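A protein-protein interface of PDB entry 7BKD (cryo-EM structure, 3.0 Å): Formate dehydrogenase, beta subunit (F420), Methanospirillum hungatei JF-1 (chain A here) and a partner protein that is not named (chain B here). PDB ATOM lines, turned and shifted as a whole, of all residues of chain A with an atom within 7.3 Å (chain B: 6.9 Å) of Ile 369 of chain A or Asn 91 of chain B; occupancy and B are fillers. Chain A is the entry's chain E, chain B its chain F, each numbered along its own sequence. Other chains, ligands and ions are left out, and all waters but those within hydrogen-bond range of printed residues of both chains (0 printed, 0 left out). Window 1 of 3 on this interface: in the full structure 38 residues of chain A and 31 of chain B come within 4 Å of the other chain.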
ATOM      1  N   PHE A 335      14.051 -21.224 -15.218  1.00  0.00           N
ATOM      2  CA  PHE A 335      13.285 -20.706 -16.346  1.00  0.00           C
ATOM      3  C   PHE A 335      12.150 -21.648 -16.711  1.00  0.00           C
ATOM      4  O   PHE A 335      11.004 -21.223 -16.880  1.00  0.00           O
ATOM      5  CB  PHE A 335      14.198 -20.496 -17.552  1.00  0.00           C
ATOM      6  CG  PHE A 335      15.143 -19.349 -17.408  1.00  0.00           C
ATOM      7  CD1 PHE A 335      14.840 -18.283 -16.591  1.00  0.00           C
ATOM      8  CD2 PHE A 335      16.334 -19.330 -18.103  1.00  0.00           C
ATOM      9  CE1 PHE A 335      15.710 -17.232 -16.462  1.00  0.00           C
ATOM     10  CE2 PHE A 335      17.204 -18.278 -17.979  1.00  0.00           C
ATOM     11  CZ  PHE A 335      16.892 -17.229 -17.158  1.00  0.00           C
ATOM     12  N   VAL A 338       9.484 -21.786 -13.549  1.00  0.00           N
ATOM     13  CA  VAL A 338       8.872 -20.597 -12.988  1.00  0.00           C
ATOM     14  C   VAL A 338       8.360 -19.630 -14.049  1.00  0.00           C
ATOM     15  O   VAL A 338       7.343 -18.968 -13.821  1.00  0.00           O
ATOM     16  CB  VAL A 338       9.852 -19.883 -12.034  1.00  0.00           C
ATOM     17  CG1 VAL A 338       9.159 -18.756 -11.309  1.00  0.00           C
ATOM     18  CG2 VAL A 338      10.437 -20.864 -11.042  1.00  0.00           C
ATOM     19  N   SER A 339       9.016 -19.541 -15.206  1.00  0.00           N
ATOM     20  CA  SER A 339       8.722 -18.462 -16.141  1.00  0.00           C
ATOM     21  C   SER A 339       7.288 -18.482 -16.643  1.00  0.00           C
ATOM     22  O   SER A 339       6.825 -17.477 -17.184  1.00  0.00           O
ATOM     23  CB  SER A 339       9.676 -18.516 -17.329  1.00  0.00           C
ATOM     24  OG  SER A 339       9.416 -19.651 -18.128  1.00  0.00           O
ATOM     25  N   ASP A 340       6.578 -19.599 -16.508  1.00  0.00           N
ATOM     26  CA  ASP A 340       5.178 -19.600 -16.906  1.00  0.00           C
ATOM     27  C   ASP A 340       4.340 -18.747 -15.966  1.00  0.00           C
ATOM     28  O   ASP A 340       3.447 -18.019 -16.413  1.00  0.00           O
ATOM     29  CB  ASP A 340       4.645 -21.032 -16.976  1.00  0.00           C
ATOM     30  CG  ASP A 340       4.673 -21.746 -15.636  1.00  0.00           C
ATOM     31  OD1 ASP A 340       5.144 -21.158 -14.640  1.00  0.00           O
ATOM     32  OD2 ASP A 340       4.208 -22.904 -15.576  1.00  0.00           O
ATOM     33  N   SER A 341       4.611 -18.816 -14.667  1.00  0.00           N
ATOM     34  CA  SER A 341       3.839 -18.095 -13.656  1.00  0.00           C
ATOM     35  C   SER A 341       4.810 -17.383 -12.727  1.00  0.00           C
ATOM     36  O   SER A 341       5.134 -17.886 -11.657  1.00  0.00           O
ATOM     37  CB  SER A 341       2.938 -19.043 -12.897  1.00  0.00           C
ATOM     38  OG  SER A 341       3.696 -20.080 -12.307  1.00  0.00           O
ATOM     39  N   MET A 362      13.509 -13.532 -15.783  1.00  0.00           N
ATOM     40  CA  MET A 362      12.316 -14.328 -15.549  1.00  0.00           C
ATOM     41  C   MET A 362      11.073 -13.616 -16.055  1.00  0.00           C
ATOM     42  O   MET A 362      10.215 -14.232 -16.695  1.00  0.00           O
ATOM     43  CB  MET A 362      12.189 -14.651 -14.065  1.00  0.00           C
ATOM     44  CG  MET A 362      11.192 -15.743 -13.764  1.00  0.00           C
ATOM     45  SD  MET A 362      11.644 -17.325 -14.474  1.00  0.00           S
ATOM     46  CE  MET A 362      13.015 -17.777 -13.433  1.00  0.00           C
ATOM     47  N   HIS A 363      10.965 -12.311 -15.805  1.00  0.00           N
ATOM     48  CA  HIS A 363       9.811 -11.570 -16.288  1.00  0.00           C
ATOM     49  C   HIS A 363       9.827 -11.463 -17.803  1.00  0.00           C
ATOM     50  O   HIS A 363       8.763 -11.386 -18.432  1.00  0.00           O
ATOM     51  CB  HIS A 363       9.788 -10.180 -15.660  1.00  0.00           C
ATOM     52  CG  HIS A 363       8.452  -9.516 -15.714  1.00  0.00           C
ATOM     53  ND1 HIS A 363       8.289  -8.157 -15.571  1.00  0.00           N
ATOM     54  CD2 HIS A 363       7.209 -10.032 -15.844  1.00  0.00           C
ATOM     55  CE1 HIS A 363       7.005  -7.860 -15.644  1.00  0.00           C
ATOM     56  NE2 HIS A 363       6.328  -8.981 -15.805  1.00  0.00           N
ATOM     57  N   SER A 364      11.018 -11.457 -18.406  1.00  0.00           N
ATOM     58  CA  SER A 364      11.101 -11.435 -19.860  1.00  0.00           C
ATOM     59  C   SER A 364      10.494 -12.689 -20.468  1.00  0.00           C
ATOM     60  O   SER A 364       9.767 -12.610 -21.461  1.00  0.00           O
ATOM     61  CB  SER A 364      12.545 -11.286 -20.304  1.00  0.00           C
ATOM     62  OG  SER A 364      13.187 -12.542 -20.362  1.00  0.00           O
ATOM     63  N   GLN A 365      10.792 -13.866 -19.907  1.00  0.00           N
ATOM     64  CA  GLN A 365      10.048 -15.020 -20.421  1.00  0.00           C
ATOM     65  C   GLN A 365       8.578 -14.964 -20.025  1.00  0.00           C
ATOM     66  O   GLN A 365       7.723 -15.423 -20.791  1.00  0.00           O
ATOM     67  CB  GLN A 365      10.611 -16.390 -20.015  1.00  0.00           C
ATOM     68  CG  GLN A 365      11.971 -16.805 -20.572  1.00  0.00           C
ATOM     69  CD  GLN A 365      13.128 -16.265 -19.806  1.00  0.00           C
ATOM     70  OE1 GLN A 365      12.973 -15.846 -18.672  1.00  0.00           O
ATOM     71  NE2 GLN A 365      14.304 -16.274 -20.416  1.00  0.00           N
ATOM     72  N   GLN A 366       8.272 -14.439 -18.838  1.00  0.00           N
ATOM     73  CA  GLN A 366       6.886 -14.356 -18.383  1.00  0.00           C
ATOM     74  C   GLN A 366       5.994 -13.634 -19.374  1.00  0.00           C
ATOM     75  O   GLN A 366       4.876 -14.077 -19.646  1.00  0.00           O
ATOM     76  CB  GLN A 366       6.811 -13.663 -17.028  1.00  0.00           C
ATOM     77  CG  GLN A 366       5.399 -13.593 -16.493  1.00  0.00           C
ATOM     78  CD  GLN A 366       4.828 -14.933 -16.168  1.00  0.00           C
ATOM     79  OE1 GLN A 366       5.507 -15.792 -15.615  1.00  0.00           O
ATOM     80  NE2 GLN A 366       3.572 -15.137 -16.534  1.00  0.00           N
ATOM     81  N   VAL A 367       6.438 -12.490 -19.879  1.00  0.00           N
ATOM     82  CA  VAL A 367       5.551 -11.694 -20.722  1.00  0.00           C
ATOM     83  C   VAL A 367       5.225 -12.440 -22.014  1.00  0.00           C
ATOM     84  O   VAL A 367       4.082 -12.425 -22.489  1.00  0.00           O
ATOM     85  CB  VAL A 367       6.161 -10.306 -20.978  1.00  0.00           C
ATOM     86  CG1 VAL A 367       6.282  -9.556 -19.672  1.00  0.00           C
ATOM     87  CG2 VAL A 367       7.511 -10.423 -21.640  1.00  0.00           C
ATOM     88  N   GLU A 368       6.213 -13.143 -22.575  1.00  0.00           N
ATOM     89  CA  GLU A 368       5.993 -13.926 -23.786  1.00  0.00           C
ATOM     90  C   GLU A 368       5.064 -15.106 -23.523  1.00  0.00           C
ATOM     91  O   GLU A 368       4.142 -15.373 -24.307  1.00  0.00           O
ATOM     92  CB  GLU A 368       7.336 -14.408 -24.325  1.00  0.00           C
ATOM     93  CG  GLU A 368       8.350 -13.298 -24.516  1.00  0.00           C
ATOM     94  CD  GLU A 368       8.087 -12.468 -25.750  1.00  0.00           C
ATOM     95  OE1 GLU A 368       7.634 -13.036 -26.766  1.00  0.00           O
ATOM     96  OE2 GLU A 368       8.329 -11.245 -25.711  1.00  0.00           O
ATOM     97  N   ILE A 369       5.296 -15.828 -22.424  1.00  0.00           N
ATOM     98  CA  ILE A 369       4.413 -16.936 -22.065  1.00  0.00           C
ATOM     99  C   ILE A 369       2.989 -16.437 -21.884  1.00  0.00           C
ATOM    100  O   ILE A 369       2.029 -17.070 -22.337  1.00  0.00           O
ATOM    101  CB  ILE A 369       4.918 -17.643 -20.792  1.00  0.00           C
ATOM    102  CG1 ILE A 369       6.327 -18.191 -20.985  1.00  0.00           C
ATOM    103  CG2 ILE A 369       3.983 -18.764 -20.400  1.00  0.00           C
ATOM    104  CD1 ILE A 369       6.423 -19.206 -22.069  1.00  0.00           C
ATOM    105  N   GLU A 370       2.832 -15.297 -21.218  1.00  0.00           N
ATOM    106  CA  GLU A 370       1.503 -14.758 -20.968  1.00  0.00           C
ATOM    107  C   GLU A 370       0.809 -14.382 -22.264  1.00  0.00           C
ATOM    108  O   GLU A 370      -0.385 -14.650 -22.433  1.00  0.00           O
ATOM    109  CB  GLU A 370       1.597 -13.545 -20.045  1.00  0.00           C
ATOM    110  CG  GLU A 370       0.279 -13.148 -19.416  1.00  0.00           C
ATOM    111  CD  GLU A 370       0.388 -11.888 -18.582  1.00  0.00           C
ATOM    112  OE1 GLU A 370       1.122 -11.902 -17.571  1.00  0.00           O
ATOM    113  OE2 GLU A 370      -0.259 -10.882 -18.939  1.00  0.00           O
ATOM    114  N   LYS A 371       1.530 -13.760 -23.195  1.00  0.00           N
ATOM    115  CA  LYS A 371       0.856 -13.362 -24.420  1.00  0.00           C
ATOM    116  C   LYS A 371       0.587 -14.535 -25.350  1.00  0.00           C
ATOM    117  O   LYS A 371      -0.304 -14.432 -26.199  1.00  0.00           O
ATOM    118  CB  LYS A 371       1.644 -12.286 -25.170  1.00  0.00           C
ATOM    119  CG  LYS A 371       2.748 -12.789 -26.066  1.00  0.00           C
ATOM    120  CD  LYS A 371       3.560 -11.618 -26.582  1.00  0.00           C
ATOM    121  CE  LYS A 371       4.689 -12.073 -27.482  1.00  0.00           C
ATOM    122  NZ  LYS A 371       5.866 -11.167 -27.386  1.00  0.00           N
ATOM    123  N   MET A 372       1.311 -15.648 -25.217  1.00  0.00           N
ATOM    124  CA  MET A 372       0.934 -16.758 -26.088  1.00  0.00           C
ATOM    125  C   MET A 372      -0.142 -17.636 -25.458  1.00  0.00           C
ATOM    126  O   MET A 372      -1.169 -17.903 -26.087  1.00  0.00           O
ATOM    127  CB  MET A 372       2.129 -17.634 -26.458  1.00  0.00           C
ATOM    128  CG  MET A 372       1.678 -18.729 -27.421  1.00  0.00           C
ATOM    129  SD  MET A 372       2.884 -19.905 -28.048  1.00  0.00           S
ATOM    130  CE  MET A 372       3.170 -20.881 -26.593  1.00  0.00           C
ATOM    131  N   PHE A 373       0.078 -18.102 -24.229  1.00  0.00           N
ATOM    132  CA  PHE A 373      -0.889 -18.979 -23.577  1.00  0.00           C
ATOM    133  C   PHE A 373      -2.083 -18.235 -22.997  1.00  0.00           C
ATOM    134  O   PHE A 373      -3.126 -18.854 -22.776  1.00  0.00           O
ATOM    135  CB  PHE A 373      -0.218 -19.777 -22.464  1.00  0.00           C
ATOM    136  CG  PHE A 373       0.718 -20.834 -22.953  1.00  0.00           C
ATOM    137  CD1 PHE A 373       0.233 -21.998 -23.507  1.00  0.00           C
ATOM    138  CD2 PHE A 373       2.081 -20.674 -22.835  1.00  0.00           C
ATOM    139  CE1 PHE A 373       1.090 -22.974 -23.951  1.00  0.00           C
ATOM    140  CE2 PHE A 373       2.942 -21.650 -23.272  1.00  0.00           C
ATOM    141  CZ  PHE A 373       2.444 -22.802 -23.831  1.00  0.00           C
ATOM    142  N   GLY A 374      -1.958 -16.937 -22.746  1.00  0.00           N
ATOM    143  CA  GLY A 374      -3.045 -16.182 -22.147  1.00  0.00           C
ATOM    144  C   GLY A 374      -3.353 -16.545 -20.710  1.00  0.00           C
ATOM    145  O   GLY A 374      -4.528 -16.614 -20.331  1.00  0.00           O
ATOM    146  N   HIS A 375      -2.324 -16.769 -19.897  1.00  0.00           N
ATOM    147  CA  HIS A 375      -2.483 -17.146 -18.497  1.00  0.00           C
ATOM    148  C   HIS A 375      -1.837 -16.069 -17.639  1.00  0.00           C
ATOM    149  O   HIS A 375      -0.610 -15.938 -17.623  1.00  0.00           O
ATOM    150  CB  HIS A 375      -1.859 -18.514 -18.233  1.00  0.00           C
ATOM    151  CG  HIS A 375      -1.762 -18.869 -16.782  1.00  0.00           C
ATOM    152  ND1 HIS A 375      -0.562 -18.918 -16.108  1.00  0.00           N
ATOM    153  CD2 HIS A 375      -2.714 -19.204 -15.879  1.00  0.00           C
ATOM    154  CE1 HIS A 375      -0.778 -19.261 -14.851  1.00  0.00           C
ATOM    155  NE2 HIS A 375      -2.076 -19.440 -14.686  1.00  0.00           N
ATOM    156  N   ILE A 385      -0.158 -23.552 -16.246  1.00  0.00           N
ATOM    157  CA  ILE A 385      -0.422 -23.966 -17.619  1.00  0.00           C
ATOM    158  C   ILE A 385      -0.128 -25.444 -17.820  1.00  0.00           C
ATOM    159  O   ILE A 385      -0.732 -26.090 -18.682  1.00  0.00           O
ATOM    160  CB  ILE A 385       0.371 -23.091 -18.608  1.00  0.00           C
ATOM    161  CG1 ILE A 385       1.866 -23.364 -18.501  1.00  0.00           C
ATOM    162  CG2 ILE A 385       0.088 -21.627 -18.363  1.00  0.00           C
ATOM    163  CD1 ILE A 385       2.661 -22.760 -19.622  1.00  0.00           C
ATOM    164  N   HIS A 386       0.785 -26.009 -17.033  1.00  0.00           N
ATOM    165  CA  HIS A 386       1.121 -27.418 -17.164  1.00  0.00           C
ATOM    166  C   HIS A 386       0.367 -28.311 -16.197  1.00  0.00           C
ATOM    167  O   HIS A 386       0.320 -29.524 -16.411  1.00  0.00           O
ATOM    168  CB  HIS A 386       2.622 -27.623 -16.967  1.00  0.00           C
ATOM    169  CG  HIS A 386       3.458 -26.862 -17.939  1.00  0.00           C
ATOM    170  ND1 HIS A 386       3.214 -26.875 -19.295  1.00  0.00           N
ATOM    171  CD2 HIS A 386       4.526 -26.053 -17.756  1.00  0.00           C
ATOM    172  CE1 HIS A 386       4.101 -26.112 -19.905  1.00  0.00           C
ATOM    173  NE2 HIS A 386       4.905 -25.598 -18.993  1.00  0.00           N
ATOM    174  N   ILE A 410       4.750 -20.078 -35.467  1.00  0.00           N
ATOM    175  CA  ILE A 410       4.157 -20.030 -34.139  1.00  0.00           C
ATOM    176  C   ILE A 410       4.122 -18.584 -33.673  1.00  0.00           C
ATOM    177  O   ILE A 410       3.181 -18.153 -33.001  1.00  0.00           O
ATOM    178  CB  ILE A 410       4.938 -20.908 -33.149  1.00  0.00           C
ATOM    179  CG1 ILE A 410       4.885 -22.370 -33.578  1.00  0.00           C
ATOM    180  CG2 ILE A 410       4.341 -20.786 -31.765  1.00  0.00           C
ATOM    181  CD1 ILE A 410       5.828 -23.248 -32.812  1.00  0.00           C
ATOM    182  N   PHE A 411       5.140 -17.822 -34.042  1.00  0.00           N
ATOM    183  CA  PHE A 411       5.355 -16.499 -33.482  1.00  0.00           C
ATOM    184  C   PHE A 411       5.282 -15.430 -34.563  1.00  0.00           C
ATOM    185  O   PHE A 411       5.293 -15.713 -35.763  1.00  0.00           O
ATOM    186  CB  PHE A 411       6.707 -16.434 -32.771  1.00  0.00           C
ATOM    187  CG  PHE A 411       6.872 -17.464 -31.695  1.00  0.00           C
ATOM    188  CD1 PHE A 411       5.937 -17.585 -30.684  1.00  0.00           C
ATOM    189  CD2 PHE A 411       7.954 -18.324 -31.706  1.00  0.00           C
ATOM    190  CE1 PHE A 411       6.082 -18.542 -29.714  1.00  0.00           C
ATOM    191  CE2 PHE A 411       8.113 -19.268 -30.725  1.00  0.00           C
ATOM    192  CZ  PHE A 411       7.175 -19.386 -29.731  1.00  0.00           C
ATOM    193  N   MET B  86       6.456 -28.621 -25.245  1.00  0.00           N
ATOM    194  CA  MET B  86       7.339 -28.238 -26.336  1.00  0.00           C
ATOM    195  C   MET B  86       7.032 -26.841 -26.857  1.00  0.00           C
ATOM    196  O   MET B  86       7.948 -26.140 -27.299  1.00  0.00           O
ATOM    197  CB  MET B  86       7.266 -29.264 -27.464  1.00  0.00           C
ATOM    198  CG  MET B  86       7.542 -30.692 -27.005  1.00  0.00           C
ATOM    199  SD  MET B  86       9.117 -30.958 -26.173  1.00  0.00           S
ATOM    200  CE  MET B  86       8.586 -31.794 -24.687  1.00  0.00           C
ATOM    201  N   PHE B  87       5.774 -26.403 -26.797  1.00  0.00           N
ATOM    202  CA  PHE B  87       5.475 -25.007 -27.097  1.00  0.00           C
ATOM    203  C   PHE B  87       6.185 -24.079 -26.117  1.00  0.00           C
ATOM    204  O   PHE B  87       6.825 -23.092 -26.516  1.00  0.00           O
ATOM    205  CB  PHE B  87       3.965 -24.772 -27.061  1.00  0.00           C
ATOM    206  CG  PHE B  87       3.282 -25.023 -28.370  1.00  0.00           C
ATOM    207  CD1 PHE B  87       3.642 -24.315 -29.499  1.00  0.00           C
ATOM    208  CD2 PHE B  87       2.279 -25.963 -28.472  1.00  0.00           C
ATOM    209  CE1 PHE B  87       3.018 -24.544 -30.704  1.00  0.00           C
ATOM    210  CE2 PHE B  87       1.651 -26.195 -29.675  1.00  0.00           C
ATOM    211  CZ  PHE B  87       2.022 -25.484 -30.792  1.00  0.00           C
ATOM    212  N   MET B  88       6.100 -24.393 -24.823  1.00  0.00           N
ATOM    213  CA  MET B  88       6.803 -23.570 -23.846  1.00  0.00           C
ATOM    214  C   MET B  88       8.313 -23.647 -24.035  1.00  0.00           C
ATOM    215  O   MET B  88       9.016 -22.654 -23.825  1.00  0.00           O
ATOM    216  CB  MET B  88       6.413 -23.978 -22.428  1.00  0.00           C
ATOM    217  CG  MET B  88       7.048 -23.107 -21.362  1.00  0.00           C
ATOM    218  SD  MET B  88       6.535 -23.505 -19.690  1.00  0.00           S
ATOM    219  CE  MET B  88       7.559 -22.367 -18.767  1.00  0.00           C
ATOM    220  N   ILE B  89       8.824 -24.805 -24.446  1.00  0.00           N
ATOM    221  CA  ILE B  89      10.248 -24.942 -24.728  1.00  0.00           C
ATOM    222  C   ILE B  89      10.659 -24.040 -25.882  1.00  0.00           C
ATOM    223  O   ILE B  89      11.730 -23.425 -25.856  1.00  0.00           O
ATOM    224  CB  ILE B  89      10.588 -26.420 -24.998  1.00  0.00           C
ATOM    225  CG1 ILE B  89      10.670 -27.186 -23.682  1.00  0.00           C
ATOM    226  CG2 ILE B  89      11.879 -26.558 -25.764  1.00  0.00           C
ATOM    227  CD1 ILE B  89      11.757 -26.680 -22.769  1.00  0.00           C
ATOM    228  N   LYS B  90       9.831 -23.959 -26.923  1.00  0.00           N
ATOM    229  CA  LYS B  90      10.152 -23.074 -28.039  1.00  0.00           C
ATOM    230  C   LYS B  90      10.180 -21.617 -27.592  1.00  0.00           C
ATOM    231  O   LYS B  90      11.080 -20.858 -27.979  1.00  0.00           O
ATOM    232  CB  LYS B  90       9.155 -23.281 -29.174  1.00  0.00           C
ATOM    233  CG  LYS B  90       9.442 -24.523 -29.992  1.00  0.00           C
ATOM    234  CD  LYS B  90       8.879 -24.418 -31.390  1.00  0.00           C
ATOM    235  CE  LYS B  90       9.897 -23.856 -32.354  1.00  0.00           C
ATOM    236  NZ  LYS B  90      10.958 -24.841 -32.667  1.00  0.00           N
ATOM    237  N   ASN B  91       9.213 -21.214 -26.761  1.00  0.00           N
ATOM    238  CA  ASN B  91       9.286 -19.885 -26.153  1.00  0.00           C
ATOM    239  C   ASN B  91      10.602 -19.678 -25.418  1.00  0.00           C
ATOM    240  O   ASN B  91      11.249 -18.634 -25.555  1.00  0.00           O
ATOM    241  CB  ASN B  91       8.132 -19.658 -25.183  1.00  0.00           C
ATOM    242  CG  ASN B  91       6.865 -19.264 -25.871  1.00  0.00           C
ATOM    243  OD1 ASN B  91       5.901 -20.013 -25.880  1.00  0.00           O
ATOM    244  ND2 ASN B  91       6.847 -18.066 -26.436  1.00  0.00           N
ATOM    245  N   LEU B  92      10.997 -20.656 -24.607  1.00  0.00           N
ATOM    246  CA  LEU B  92      12.180 -20.489 -23.775  1.00  0.00           C
ATOM    247  C   LEU B  92      13.437 -20.354 -24.625  1.00  0.00           C
ATOM    248  O   LEU B  92      14.270 -19.476 -24.374  1.00  0.00           O
ATOM    249  CB  LEU B  92      12.290 -21.661 -22.802  1.00  0.00           C
ATOM    250  CG  LEU B  92      13.322 -21.637 -21.675  1.00  0.00           C
ATOM    251  CD1 LEU B  92      12.815 -22.489 -20.541  1.00  0.00           C
ATOM    252  CD2 LEU B  92      14.680 -22.134 -22.129  1.00  0.00           C
ATOM    253  N   LEU B  93      13.586 -21.204 -25.643  1.00  0.00           N
ATOM    254  CA  LEU B  93      14.756 -21.099 -26.511  1.00  0.00           C
ATOM    255  C   LEU B  93      14.778 -19.807 -27.312  1.00  0.00           C
ATOM    256  O   LEU B  93      15.859 -19.275 -27.582  1.00  0.00           O
ATOM    257  CB  LEU B  93      14.883 -22.304 -27.441  1.00  0.00           C
ATOM    258  CG  LEU B  93      15.455 -23.612 -26.897  1.00  0.00           C
ATOM    259  CD1 LEU B  93      14.563 -24.352 -25.950  1.00  0.00           C
ATOM    260  CD2 LEU B  93      15.791 -24.479 -28.091  1.00  0.00           C
ATOM    261  N   ARG B  94      13.622 -19.281 -27.727  1.00  0.00           N
ATOM    262  CA  ARG B  94      13.687 -17.959 -28.344  1.00  0.00           C
ATOM    263  C   ARG B  94      14.119 -16.900 -27.339  1.00  0.00           C
ATOM    264  O   ARG B  94      15.020 -16.100 -27.615  1.00  0.00           O
ATOM    265  CB  ARG B  94      12.372 -17.545 -29.002  1.00  0.00           C
ATOM    266  CG  ARG B  94      12.597 -16.181 -29.646  1.00  0.00           C
ATOM    267  CD  ARG B  94      11.476 -15.548 -30.443  1.00  0.00           C
ATOM    268  NE  ARG B  94      11.173 -16.249 -31.682  1.00  0.00           N
ATOM    269  CZ  ARG B  94      10.132 -15.957 -32.447  1.00  0.00           C
ATOM    270  NH1 ARG B  94       9.334 -14.954 -32.103  1.00  0.00           N
ATOM    271  NH2 ARG B  94       9.917 -16.635 -33.570  1.00  0.00           N
ATOM    272  N   ASN B  95      13.519 -16.904 -26.150  1.00  0.00           N
ATOM    273  CA  ASN B  95      13.724 -15.793 -25.233  1.00  0.00           C
ATOM    274  C   ASN B  95      15.079 -15.833 -24.546  1.00  0.00           C
ATOM    275  O   ASN B  95      15.481 -14.828 -23.956  1.00  0.00           O
ATOM    276  CB  ASN B  95      12.616 -15.772 -24.189  1.00  0.00           C
ATOM    277  CG  ASN B  95      11.299 -15.338 -24.765  1.00  0.00           C
ATOM    278  OD1 ASN B  95      11.235 -14.398 -25.550  1.00  0.00           O
ATOM    279  ND2 ASN B  95      10.234 -16.029 -24.389  1.00  0.00           N
ATOM    280  N   ILE B  96      15.791 -16.963 -24.592  1.00  0.00           N
ATOM    281  CA  ILE B  96      17.151 -16.991 -24.068  1.00  0.00           C
ATOM    282  C   ILE B  96      18.190 -16.703 -25.137  1.00  0.00           C
ATOM    283  O   ILE B  96      19.391 -16.773 -24.851  1.00  0.00           O
ATOM    284  CB  ILE B  96      17.495 -18.335 -23.397  1.00  0.00           C
ATOM    285  CG1 ILE B  96      17.488 -19.465 -24.423  1.00  0.00           C
ATOM    286  CG2 ILE B  96      16.543 -18.620 -22.254  1.00  0.00           C
ATOM    287  CD1 ILE B  96      18.224 -20.697 -23.969  1.00  0.00           C
ATOM    288  N   ASP B 100      15.158 -20.935 -31.952  1.00  0.00           N
ATOM    289  CA  ASP B 100      14.086 -21.866 -31.624  1.00  0.00           C
ATOM    290  C   ASP B 100      13.821 -22.873 -32.732  1.00  0.00           C
ATOM    291  O   ASP B 100      13.074 -23.828 -32.508  1.00  0.00           O
ATOM    292  CB  ASP B 100      12.802 -21.103 -31.295  1.00  0.00           C
ATOM    293  CG  ASP B 100      12.263 -20.323 -32.476  1.00  0.00           C
ATOM    294  OD1 ASP B 100      11.070 -20.494 -32.803  1.00  0.00           O
ATOM    295  OD2 ASP B 100      13.027 -19.536 -33.075  1.00  0.00           O
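A ring nitrogen (NE2) of His 386 of chain A lies within hydrogen-bond range of the side-chain sulfur of Met 88 of chain B, at 2.7 Å. The side-chain amide oxygen (OD1) of Asn 91 of chain B sits close to the side-chain sulfur (SD) of Met 372 of chain A, 3.7 Å away.
The backbone carbonyl oxygen (O) of Phe 87 of chain B sits close to the side-chain amide oxygen (OD1) of Asn 91 of chain B (3.3 Å). The side-chain amide nitrogen of Asn 95 of chain B sits at hydrogen-bond distance from the backbone carbonyl oxygen of Asn 91 of chain B (3.0 Å). The backbone NH of Ser 339 of chain A sits at hydrogen-bond distance from the side-chain sulfur of Met 362 of chain A (3.5 Å). OG of Ser 341 of chain A is in hydrogen-bond range of OD1 of Asp 340 of chain A (2.9 Å). The backbone carbonyl oxygen of Asp 340 of chain A lies within hydrogen-bond range of the side-chain amide nitrogen of Gln 366 of chain A, at 2.9 Å. NZ of Lys 371 of chain A lies within salt-bridge range of OE1 of Glu 368 of chain A (2.6 Å).
Phe 335 of chain A touches Leu 92 of chain B (CB to CD1, 3.8 Å). Ser 339 of chain A touches Met 88 of chain B. CG of Gln 365 of chain A touches CB of Asn 95 of chain B, at 3.8 Å. CG of Glu 368 of chain A touches OD1 of Asn 95 of chain B, at 3.3 Å. CD1 of Ile 369 of chain A touches CB of Asn 91 of chain B, at 3.6 Å. Phe 87 of chain B touches Met 372 of chain A (CB to CE, 3.999 Å). Phe 87 of chain B touches Ile 410 of chain A. Phe 411 of chain A touches Asn 91 of chain B. Arg 94 of chain B touches Phe 411 of chain A (NH1 to CB, 3.1 Å). Phe 411 of chain A touches Asp 100 of chain B.
Of the printed residues of chain B, Ile 369 of chain A touches Asn 91. Of chain A, only Ile 369 (3.6 Å), Met 372 (3.0 Å) and Phe 411 (3.4 Å) come within 4 Å of Asn 91 of chain B. Printed residues of chain B within 4 Å of Asp 340 of chain A: Met 88 (3.7 Å). Of the printed residues of chain A, Ile 96 of chain B touches Gln 365. Of the printed residues of chain A, Lys 90 of chain B touches Ile 410 (3.6 Å). Of the printed residues of chain B, Met 372 of chain A touches Phe 87 and Asn 91. Of the printed residues of chain B, His 386 of chain A touches Met 88. Gln 366 of chain A touches none of the printed residues of chain B. Ser 364 of chain A touches none of the printed residues of chain B. The nearest printed residue of chain B that does not touch Ile 369 of chain A is Met 88 of chain B (4.01 Å). The nearest printed residue of chain A that does not touch Arg 94 of chain B is Glu 368 of chain A (5.9 Å).
Of the 23 printed residues of chain A, 11 touch a printed residue of chain B. Hydrophobic or aromatic side chains of chain A that line the printed part of chain B: Phe 335, Ile 369, Met 372, Ile 385, His 386, Ile 410 and Phe 411. Among the printed residues, 16 pairs touch across the chains. Among the printed residues, no Asp or Glu carboxylate lies within 4 Å of a Lys or Arg side-chain nitrogen of the other chain.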
